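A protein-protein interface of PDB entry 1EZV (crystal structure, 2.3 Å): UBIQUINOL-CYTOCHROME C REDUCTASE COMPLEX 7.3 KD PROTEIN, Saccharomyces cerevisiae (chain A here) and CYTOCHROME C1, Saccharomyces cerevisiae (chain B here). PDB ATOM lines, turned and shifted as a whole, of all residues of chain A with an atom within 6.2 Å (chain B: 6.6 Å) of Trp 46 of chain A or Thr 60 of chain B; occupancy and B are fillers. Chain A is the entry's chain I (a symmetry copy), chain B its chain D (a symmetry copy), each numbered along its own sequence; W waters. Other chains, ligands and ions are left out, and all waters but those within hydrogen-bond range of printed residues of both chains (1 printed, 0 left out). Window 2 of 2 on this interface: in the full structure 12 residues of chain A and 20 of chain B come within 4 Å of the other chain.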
ATOM      1  N   LYS A  44       7.190  28.750  17.253  1.00  0.00           N
ATOM      2  CA  LYS A  44       7.006  28.359  18.647  1.00  0.00           C
ATOM      3  C   LYS A  44       5.644  27.742  18.919  1.00  0.00           C
ATOM      4  O   LYS A  44       5.493  26.960  19.857  1.00  0.00           O
ATOM      5  CB  LYS A  44       7.211  29.569  19.555  1.00  0.00           C
ATOM      6  CG  LYS A  44       8.658  30.000  19.691  1.00  0.00           C
ATOM      7  CD  LYS A  44       8.783  31.508  19.839  1.00  0.00           C
ATOM      8  CE  LYS A  44       8.296  31.980  21.190  1.00  0.00           C
ATOM      9  NZ  LYS A  44       8.326  33.462  21.291  1.00  0.00           N
ATOM     10  N   LEU A  45       4.665  28.082  18.083  1.00  0.00           N
ATOM     11  CA  LEU A  45       3.284  27.618  18.250  1.00  0.00           C
ATOM     12  C   LEU A  45       3.128  26.108  18.103  1.00  0.00           C
ATOM     13  O   LEU A  45       3.954  25.445  17.472  1.00  0.00           O
ATOM     14  CB  LEU A  45       2.370  28.307  17.234  1.00  0.00           C
ATOM     15  CG  LEU A  45       1.655  29.613  17.586  1.00  0.00           C
ATOM     16  CD1 LEU A  45       2.189  30.207  18.889  1.00  0.00           C
ATOM     17  CD2 LEU A  45       1.822  30.587  16.426  1.00  0.00           C
ATOM     18  N   TRP A  46       2.040  25.578  18.652  1.00  0.00           N
ATOM     19  CA  TRP A  46       1.659  24.189  18.406  1.00  0.00           C
ATOM     20  C   TRP A  46       1.313  23.936  16.929  1.00  0.00           C
ATOM     21  O   TRP A  46       1.573  22.853  16.411  1.00  0.00           O
ATOM     22  CB  TRP A  46       0.474  23.796  19.291  1.00  0.00           C
ATOM     23  CG  TRP A  46      -0.054  22.427  18.998  1.00  0.00           C
ATOM     24  CD1 TRP A  46      -1.310  22.106  18.569  1.00  0.00           C
ATOM     25  CD2 TRP A  46       0.667  21.190  19.095  1.00  0.00           C
ATOM     26  NE1 TRP A  46      -1.419  20.746  18.399  1.00  0.00           N
ATOM     27  CE2 TRP A  46      -0.224  20.161  18.719  1.00  0.00           C
ATOM     28  CE3 TRP A  46       1.977  20.855  19.463  1.00  0.00           C
ATOM     29  CZ2 TRP A  46       0.155  18.812  18.704  1.00  0.00           C
ATOM     30  CZ3 TRP A  46       2.353  19.516  19.447  1.00  0.00           C
ATOM     31  CH2 TRP A  46       1.442  18.511  19.070  1.00  0.00           C
ATOM     32  N   LYS A  47       0.691  24.921  16.278  1.00  0.00           N
ATOM     33  CA  LYS A  47       0.442  24.884  14.832  1.00  0.00           C
ATOM     34  C   LYS A  47       1.702  24.481  14.078  1.00  0.00           C
ATOM     35  O   LYS A  47       1.666  23.616  13.206  1.00  0.00           O
ATOM     36  CB  LYS A  47       0.004  26.261  14.314  1.00  0.00           C
ATOM     37  CG  LYS A  47      -1.401  26.697  14.698  1.00  0.00           C
ATOM     38  CD  LYS A  47      -1.921  27.786  13.751  1.00  0.00           C
ATOM     39  CE  LYS A  47      -0.893  28.902  13.527  1.00  0.00           C
ATOM     40  NZ  LYS A  47      -1.396  29.994  12.635  1.00  0.00           N
ATOM     41  N   ASP A  48       2.818  25.105  14.449  1.00  0.00           N
ATOM     42  CA  ASP A  48       4.078  24.950  13.738  1.00  0.00           C
ATOM     43  C   ASP A  48       4.782  23.653  14.111  1.00  0.00           C
ATOM     44  O   ASP A  48       5.454  23.044  13.280  1.00  0.00           O
ATOM     45  CB  ASP A  48       4.993  26.146  14.026  1.00  0.00           C
ATOM     46  CG  ASP A  48       4.303  27.484  13.782  1.00  0.00           C
ATOM     47  OD1 ASP A  48       4.597  28.448  14.519  1.00  0.00           O
ATOM     48  OD2 ASP A  48       3.453  27.573  12.870  1.00  0.00           O
ATOM     49  N   VAL A  49       4.591  23.213  15.348  1.00  0.00           N
ATOM     50  CA  VAL A  49       5.216  21.986  15.830  1.00  0.00           C
ATOM     51  C   VAL A  49       4.524  20.751  15.253  1.00  0.00           C
ATOM     52  O   VAL A  49       5.184  19.760  14.935  1.00  0.00           O
ATOM     53  CB  VAL A  49       5.193  21.922  17.378  1.00  0.00           C
ATOM     54  CG1 VAL A  49       5.770  20.602  17.870  1.00  0.00           C
ATOM     55  CG2 VAL A  49       5.987  23.082  17.953  1.00  0.00           C
ATOM     56  N   LYS A  50       3.211  20.843  15.055  1.00  0.00           N
ATOM     57  CA  LYS A  50       2.428  19.723  14.535  1.00  0.00           C
ATOM     58  C   LYS A  50       2.781  19.413  13.081  1.00  0.00           C
ATOM     59  O   LYS A  50       2.610  18.282  12.618  1.00  0.00           O
ATOM     60  CB  LYS A  50       0.930  20.016  14.648  1.00  0.00           C
ATOM     61  CG  LYS A  50       0.068  18.761  14.639  1.00  0.00           C
ATOM     62  CD  LYS A  50      -1.390  19.069  14.332  1.00  0.00           C
ATOM     63  CE  LYS A  50      -2.213  17.785  14.265  1.00  0.00           C
ATOM     64  NZ  LYS A  50      -3.646  18.037  13.933  1.00  0.00           N
ATOM     65  N   ALA A  51       3.305  20.417  12.380  1.00  0.00           N
ATOM     66  CA  ALA A  51       3.739  20.266  10.992  1.00  0.00           C
ATOM     67  C   ALA A  51       5.021  19.437  10.878  1.00  0.00           C
ATOM     68  O   ALA A  51       5.424  19.056   9.778  1.00  0.00           O
ATOM     69  CB  ALA A  51       3.944  21.641  10.360  1.00  0.00           C
ATOM     70  N   ILE A  53       5.508  16.661  13.013  1.00  0.00           N
ATOM     71  CA  ILE A  53       5.196  15.391  13.671  1.00  0.00           C
ATOM     72  C   ILE A  53       4.126  14.665  12.849  1.00  0.00           C
ATOM     73  O   ILE A  53       3.278  15.309  12.224  1.00  0.00           O
ATOM     74  CB  ILE A  53       4.650  15.615  15.116  1.00  0.00           C
ATOM     75  CG1 ILE A  53       5.493  16.662  15.859  1.00  0.00           C
ATOM     76  CG2 ILE A  53       4.644  14.299  15.891  1.00  0.00           C
ATOM     77  CD1 ILE A  53       6.886  16.197  16.259  1.00  0.00           C
ATOM     78  N   PHE B  24       5.022  30.684  24.803  1.00  0.00           N
ATOM     79  CA  PHE B  24       5.903  29.555  25.069  1.00  0.00           C
ATOM     80  C   PHE B  24       6.416  28.985  23.742  1.00  0.00           C
ATOM     81  O   PHE B  24       5.768  29.126  22.697  1.00  0.00           O
ATOM     82  CB  PHE B  24       5.158  28.441  25.810  1.00  0.00           C
ATOM     83  CG  PHE B  24       4.907  28.727  27.260  1.00  0.00           C
ATOM     84  CD1 PHE B  24       3.671  28.423  27.830  1.00  0.00           C
ATOM     85  CD2 PHE B  24       5.922  29.200  28.080  1.00  0.00           C
ATOM     86  CE1 PHE B  24       3.460  28.572  29.196  1.00  0.00           C
ATOM     87  CE2 PHE B  24       5.716  29.357  29.451  1.00  0.00           C
ATOM     88  CZ  PHE B  24       4.486  29.039  30.007  1.00  0.00           C
ATOM     89  N   HIS B  26       6.471  25.646  22.166  1.00  0.00           N
ATOM     90  CA  HIS B  26       5.730  24.414  22.403  1.00  0.00           C
ATOM     91  C   HIS B  26       6.496  23.129  22.107  1.00  0.00           C
ATOM     92  O   HIS B  26       6.190  22.080  22.678  1.00  0.00           O
ATOM     93  CB  HIS B  26       4.417  24.444  21.626  1.00  0.00           C
ATOM     94  CG  HIS B  26       3.422  25.413  22.181  1.00  0.00           C
ATOM     95  ND1 HIS B  26       2.375  25.022  22.988  1.00  0.00           N
ATOM     96  CD2 HIS B  26       3.381  26.767  22.143  1.00  0.00           C
ATOM     97  CE1 HIS B  26       1.738  26.092  23.426  1.00  0.00           C
ATOM     98  NE2 HIS B  26       2.328  27.163  22.930  1.00  0.00           N
ATOM     99  N   ALA B  27       7.536  23.222  21.279  1.00  0.00           N
ATOM    100  CA  ALA B  27       8.445  22.094  21.059  1.00  0.00           C
ATOM    101  C   ALA B  27       9.269  21.812  22.315  1.00  0.00           C
ATOM    102  O   ALA B  27       9.422  20.656  22.727  1.00  0.00           O
ATOM    103  CB  ALA B  27       9.367  22.379  19.875  1.00  0.00           C
ATOM    104  N   ARG B  30       6.929  20.078  24.710  1.00  0.00           N
ATOM    105  CA  ARG B  30       6.869  18.666  24.319  1.00  0.00           C
ATOM    106  C   ARG B  30       8.058  17.858  24.836  1.00  0.00           C
ATOM    107  O   ARG B  30       7.880  16.848  25.511  1.00  0.00           O
ATOM    108  CB  ARG B  30       6.784  18.525  22.794  1.00  0.00           C
ATOM    109  CG  ARG B  30       6.626  17.080  22.345  1.00  0.00           C
ATOM    110  CD  ARG B  30       6.463  16.947  20.839  1.00  0.00           C
ATOM    111  NE  ARG B  30       6.350  15.542  20.452  1.00  0.00           N
ATOM    112  CZ  ARG B  30       5.208  14.926  20.167  1.00  0.00           C
ATOM    113  NH1 ARG B  30       5.216  13.630  19.883  1.00  0.00           N
ATOM    114  NH2 ARG B  30       4.068  15.603  20.109  1.00  0.00           N
ATOM    115  N   LEU B  54      -2.861  18.669  27.881  1.00  0.00           N
ATOM    116  CA  LEU B  54      -1.731  18.436  26.984  1.00  0.00           C
ATOM    117  C   LEU B  54      -2.150  18.550  25.512  1.00  0.00           C
ATOM    118  O   LEU B  54      -1.423  19.106  24.687  1.00  0.00           O
ATOM    119  CB  LEU B  54      -1.133  17.053  27.255  1.00  0.00           C
ATOM    120  CG  LEU B  54       0.108  16.959  28.152  1.00  0.00           C
ATOM    121  CD1 LEU B  54      -0.130  17.648  29.483  1.00  0.00           C
ATOM    122  CD2 LEU B  54       0.450  15.488  28.382  1.00  0.00           C
ATOM    123  N   VAL B  55      -3.381  18.142  25.221  1.00  0.00           N
ATOM    124  CA  VAL B  55      -3.876  18.123  23.853  1.00  0.00           C
ATOM    125  C   VAL B  55      -3.901  19.517  23.244  1.00  0.00           C
ATOM    126  O   VAL B  55      -4.506  20.437  23.790  1.00  0.00           O
ATOM    127  CB  VAL B  55      -5.285  17.517  23.790  1.00  0.00           C
ATOM    128  CG1 VAL B  55      -5.828  17.580  22.368  1.00  0.00           C
ATOM    129  CG2 VAL B  55      -5.250  16.087  24.291  1.00  0.00           C
ATOM    130  N   GLY B  56      -3.228  19.667  22.110  1.00  0.00           N
ATOM    131  CA  GLY B  56      -3.223  20.942  21.424  1.00  0.00           C
ATOM    132  C   GLY B  56      -2.153  21.868  21.955  1.00  0.00           C
ATOM    133  O   GLY B  56      -2.022  23.002  21.486  1.00  0.00           O
ATOM    134  N   VAL B  57      -1.414  21.403  22.963  1.00  0.00           N
ATOM    135  CA  VAL B  57      -0.342  22.197  23.552  1.00  0.00           C
ATOM    136  C   VAL B  57       1.012  21.611  23.186  1.00  0.00           C
ATOM    137  O   VAL B  57       1.868  22.301  22.626  1.00  0.00           O
ATOM    138  CB  VAL B  57      -0.461  22.269  25.101  1.00  0.00           C
ATOM    139  CG1 VAL B  57       0.768  22.961  25.699  1.00  0.00           C
ATOM    140  CG2 VAL B  57      -1.731  23.012  25.490  1.00  0.00           C
ATOM    141  N   SER B  58       1.193  20.334  23.512  1.00  0.00           N
ATOM    142  CA  SER B  58       2.463  19.654  23.312  1.00  0.00           C
ATOM    143  C   SER B  58       2.285  18.300  22.616  1.00  0.00           C
ATOM    144  O   SER B  58       3.247  17.726  22.112  1.00  0.00           O
ATOM    145  CB  SER B  58       3.154  19.454  24.662  1.00  0.00           C
ATOM    146  OG  SER B  58       2.326  18.728  25.548  1.00  0.00           O
ATOM    147  N   HIS B  59       1.056  17.791  22.612  1.00  0.00           N
ATOM    148  CA  HIS B  59       0.752  16.484  22.047  1.00  0.00           C
ATOM    149  C   HIS B  59      -0.592  16.477  21.320  1.00  0.00           C
ATOM    150  O   HIS B  59      -1.394  17.401  21.465  1.00  0.00           O
ATOM    151  CB  HIS B  59       0.736  15.426  23.150  1.00  0.00           C
ATOM    152  CG  HIS B  59       2.059  15.235  23.821  1.00  0.00           C
ATOM    153  ND1 HIS B  59       2.537  16.101  24.781  1.00  0.00           N
ATOM    154  CD2 HIS B  59       2.979  14.248  23.715  1.00  0.00           C
ATOM    155  CE1 HIS B  59       3.687  15.649  25.245  1.00  0.00           C
ATOM    156  NE2 HIS B  59       3.978  14.524  24.616  1.00  0.00           N
ATOM    157  N   THR B  60      -0.829  15.433  20.534  1.00  0.00           N
ATOM    158  CA  THR B  60      -2.101  15.277  19.835  1.00  0.00           C
ATOM    159  C   THR B  60      -3.118  14.565  20.727  1.00  0.00           C
ATOM    160  O   THR B  60      -2.753  13.888  21.695  1.00  0.00           O
ATOM    161  CB  THR B  60      -1.939  14.464  18.515  1.00  0.00           C
ATOM    162  OG1 THR B  60      -1.553  13.117  18.822  1.00  0.00           O
ATOM    163  CG2 THR B  60      -0.878  15.093  17.616  1.00  0.00           C
ATOM    164  N   ASN B  61      -4.386  14.654  20.342  1.00  0.00           N
ATOM    165  CA  ASN B  61      -5.458  13.969  21.051  1.00  0.00           C
ATOM    166  C   ASN B  61      -5.169  12.475  21.197  1.00  0.00           C
ATOM    167  O   ASN B  61      -5.359  11.901  22.270  1.00  0.00           O
ATOM    168  CB  ASN B  61      -6.789  14.179  20.319  1.00  0.00           C
ATOM    169  CG  ASN B  61      -7.987  13.927  21.211  1.00  0.00           C
ATOM    170  OD1 ASN B  61      -8.321  12.777  21.517  1.00  0.00           O
ATOM    171  ND2 ASN B  61      -8.610  15.006  21.686  1.00  0.00           N
ATOM    172  N   GLU B  62      -4.603  11.887  20.142  1.00  0.00           N
ATOM    173  CA  GLU B  62      -4.305  10.455  20.097  1.00  0.00           C
ATOM    174  C   GLU B  62      -3.158  10.075  21.030  1.00  0.00           C
ATOM    175  O   GLU B  62      -3.280   9.129  21.815  1.00  0.00           O
ATOM    176  CB  GLU B  62      -3.967  10.025  18.662  1.00  0.00           C
ATOM    177  CG  GLU B  62      -5.143  10.084  17.674  1.00  0.00           C
ATOM    178  CD  GLU B  62      -5.565  11.509  17.309  1.00  0.00           C
ATOM    179  OE1 GLU B  62      -4.680  12.377  17.123  1.00  0.00           O
ATOM    180  OE2 GLU B  62      -6.787  11.754  17.194  1.00  0.00           O
ATOM    181  N   GLU B  63      -2.067  10.839  20.966  1.00  0.00           N
ATOM    182  CA  GLU B  63      -0.895  10.611  21.816  1.00  0.00           C
ATOM    183  C   GLU B  63      -1.223  10.640  23.308  1.00  0.00           C
ATOM    184  O   GLU B  63      -0.762   9.786  24.069  1.00  0.00           O
ATOM    185  CB  GLU B  63       0.183  11.654  21.530  1.00  0.00           C
ATOM    186  CG  GLU B  63       0.704  11.634  20.114  1.00  0.00           C
ATOM    187  CD  GLU B  63       1.913  12.521  19.937  1.00  0.00           C
ATOM    188  OE1 GLU B  63       3.044  11.995  20.002  1.00  0.00           O
ATOM    189  OE2 GLU B  63       1.734  13.744  19.747  1.00  0.00           O
ATOM    190  N   VAL B  64      -2.002  11.638  23.722  1.00  0.00           N
ATOM    191  CA  VAL B  64      -2.381  11.777  25.121  1.00  0.00           C
ATOM    192  C   VAL B  64      -3.252  10.607  25.570  1.00  0.00           C
ATOM    193  O   VAL B  64      -3.086  10.092  26.674  1.00  0.00           O
ATOM    194  CB  VAL B  64      -3.129  13.116  25.374  1.00  0.00           C
ATOM    195  CG1 VAL B  64      -3.564  13.218  26.822  1.00  0.00           C
ATOM    196  CG2 VAL B  64      -2.228  14.285  25.027  1.00  0.00           C
ATOM    197  N   ARG B  65      -4.139  10.150  24.692  1.00  0.00           N
ATOM    198  CA  ARG B  65      -5.010   9.029  25.023  1.00  0.00           C
ATOM    199  C   ARG B  65      -4.205   7.759  25.289  1.00  0.00           C
ATOM    200  O   ARG B  65      -4.444   7.069  26.282  1.00  0.00           O
ATOM    201  CB  ARG B  65      -6.028   8.786  23.906  1.00  0.00           C
ATOM    202  CG  ARG B  65      -7.058   7.718  24.251  1.00  0.00           C
ATOM    203  CD  ARG B  65      -8.176   7.655  23.225  1.00  0.00           C
ATOM    204  NE  ARG B  65      -9.206   8.664  23.480  1.00  0.00           N
ATOM    205  CZ  ARG B  65      -9.446   9.713  22.694  1.00  0.00           C
ATOM    206  NH1 ARG B  65     -10.416  10.566  23.005  1.00  0.00           N
ATOM    207  NH2 ARG B  65      -8.717   9.914  21.601  1.00  0.00           N
ATOM    208  N   MET B  67      -1.068   7.671  26.278  1.00  0.00           N
ATOM    209  CA  MET B  67      -0.314   7.926  27.502  1.00  0.00           C
ATOM    210  C   MET B  67      -1.144   7.717  28.762  1.00  0.00           C
ATOM    211  O   MET B  67      -0.649   7.167  29.750  1.00  0.00           O
ATOM    212  CB  MET B  67       0.243   9.345  27.492  1.00  0.00           C
ATOM    213  CG  MET B  67       1.379   9.542  26.521  1.00  0.00           C
ATOM    214  SD  MET B  67       2.211  11.098  26.792  1.00  0.00           S
ATOM    215  CE  MET B  67       1.289  12.162  25.690  1.00  0.00           C
HETATM  216  O   HOH W   1       0.176  26.945  20.289  1.00  0.00           O
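Water W1 lies within hydrogen-bond range of the backbone NH (N) of Trp 46 of chain A (2.8 Å) and a ring nitrogen (NE2) of His 26 of chain B (3.4 Å).
Of the 9 printed residues of chain A, 4 touch a printed residue of chain B. Along chain A the printed residues that touch a printed residue of chain B span positions 44 to 49. Of the 17 printed residues of chain B, 8 touch a printed residue of chain A. Hydrophobic or aromatic side chains of chain B that line the printed part of chain A: His 26 and Ala 27. Among the printed residues, 10 pairs touch across the chains.
Of chain B, only His 26, Gly 56, Val 57, Ser 58, His 59 and Thr 60 come within 4 Å of Trp 46 of chain A. Thr 60 of chain B touches just one residue of chain A: Trp 46. Printed residues of chain B within 4 Å of Val 49 of chain A: Ala 27. Printed residues of chain A within 4 Å of His 26 of chain B: Lys 44, Leu 45 and Trp 46. Of the printed residues of chain A, Ser 58 of chain B touches Trp 46. Printed residues of chain B within 4 Å of Lys 44 of chain A: Phe 24 and His 26. Printed residues of chain B within 4 Å of Leu 45 of chain A: His 26. Asn 61 of chain B touches none of the printed residues of chain A. The nearest printed residue of chain A that does not touch His 59 of chain B is Lys 50 of chain A (7.1 Å).
ND1 of His 26 of chain B sits at hydrogen-bond distance from O of Val 57 of chain B (2.8 Å). NH2 of Arg 30 of chain B lies within hydrogen-bond range of O of Ser 58 of chain B (3.0 Å). The backbone carbonyl oxygen (O) of Leu 54 of chain B is in hydrogen-bond range of the backbone NH (N) of His 59 of chain B, 3.5 Å away. The side-chain hydroxyl of Ser 58 of chain B is in hydrogen-bond range of a ring nitrogen (ND1) of His 59 of chain B (2.7 Å). OE2 of Glu 63 of chain B is in hydrogen-bond range of N of Thr 60 of chain B (3.2 Å).
Among the printed residues, merely in contact across the chains: Lys 44 of chain A with Phe 24 of chain B (3.5 Å), Leu 45 of chain A with His 26 of chain B (3.99 Å), Trp 46 of chain A with His 26 of chain B (3.8 Å), Trp 46 of chain A with Gly 56 of chain B (3.1 Å), Trp 46 of chain A with Val 57 of chain B (3.5 Å), Trp 46 of chain A with Ser 58 of chain B (3.3 Å), Trp 46 of chain A with His 59 of chain B (3.5 Å), Trp 46 of chain A with Thr 60 of chain B (3.97 Å) and Val 49 of chain A with Ala 27 of chain B (3.7 Å).
The backbone carbonyl oxygen of Lys 44 of chain A lies within hydrogen-bond range of the backbone NH of His 26 of chain B, 2.8 Å away.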
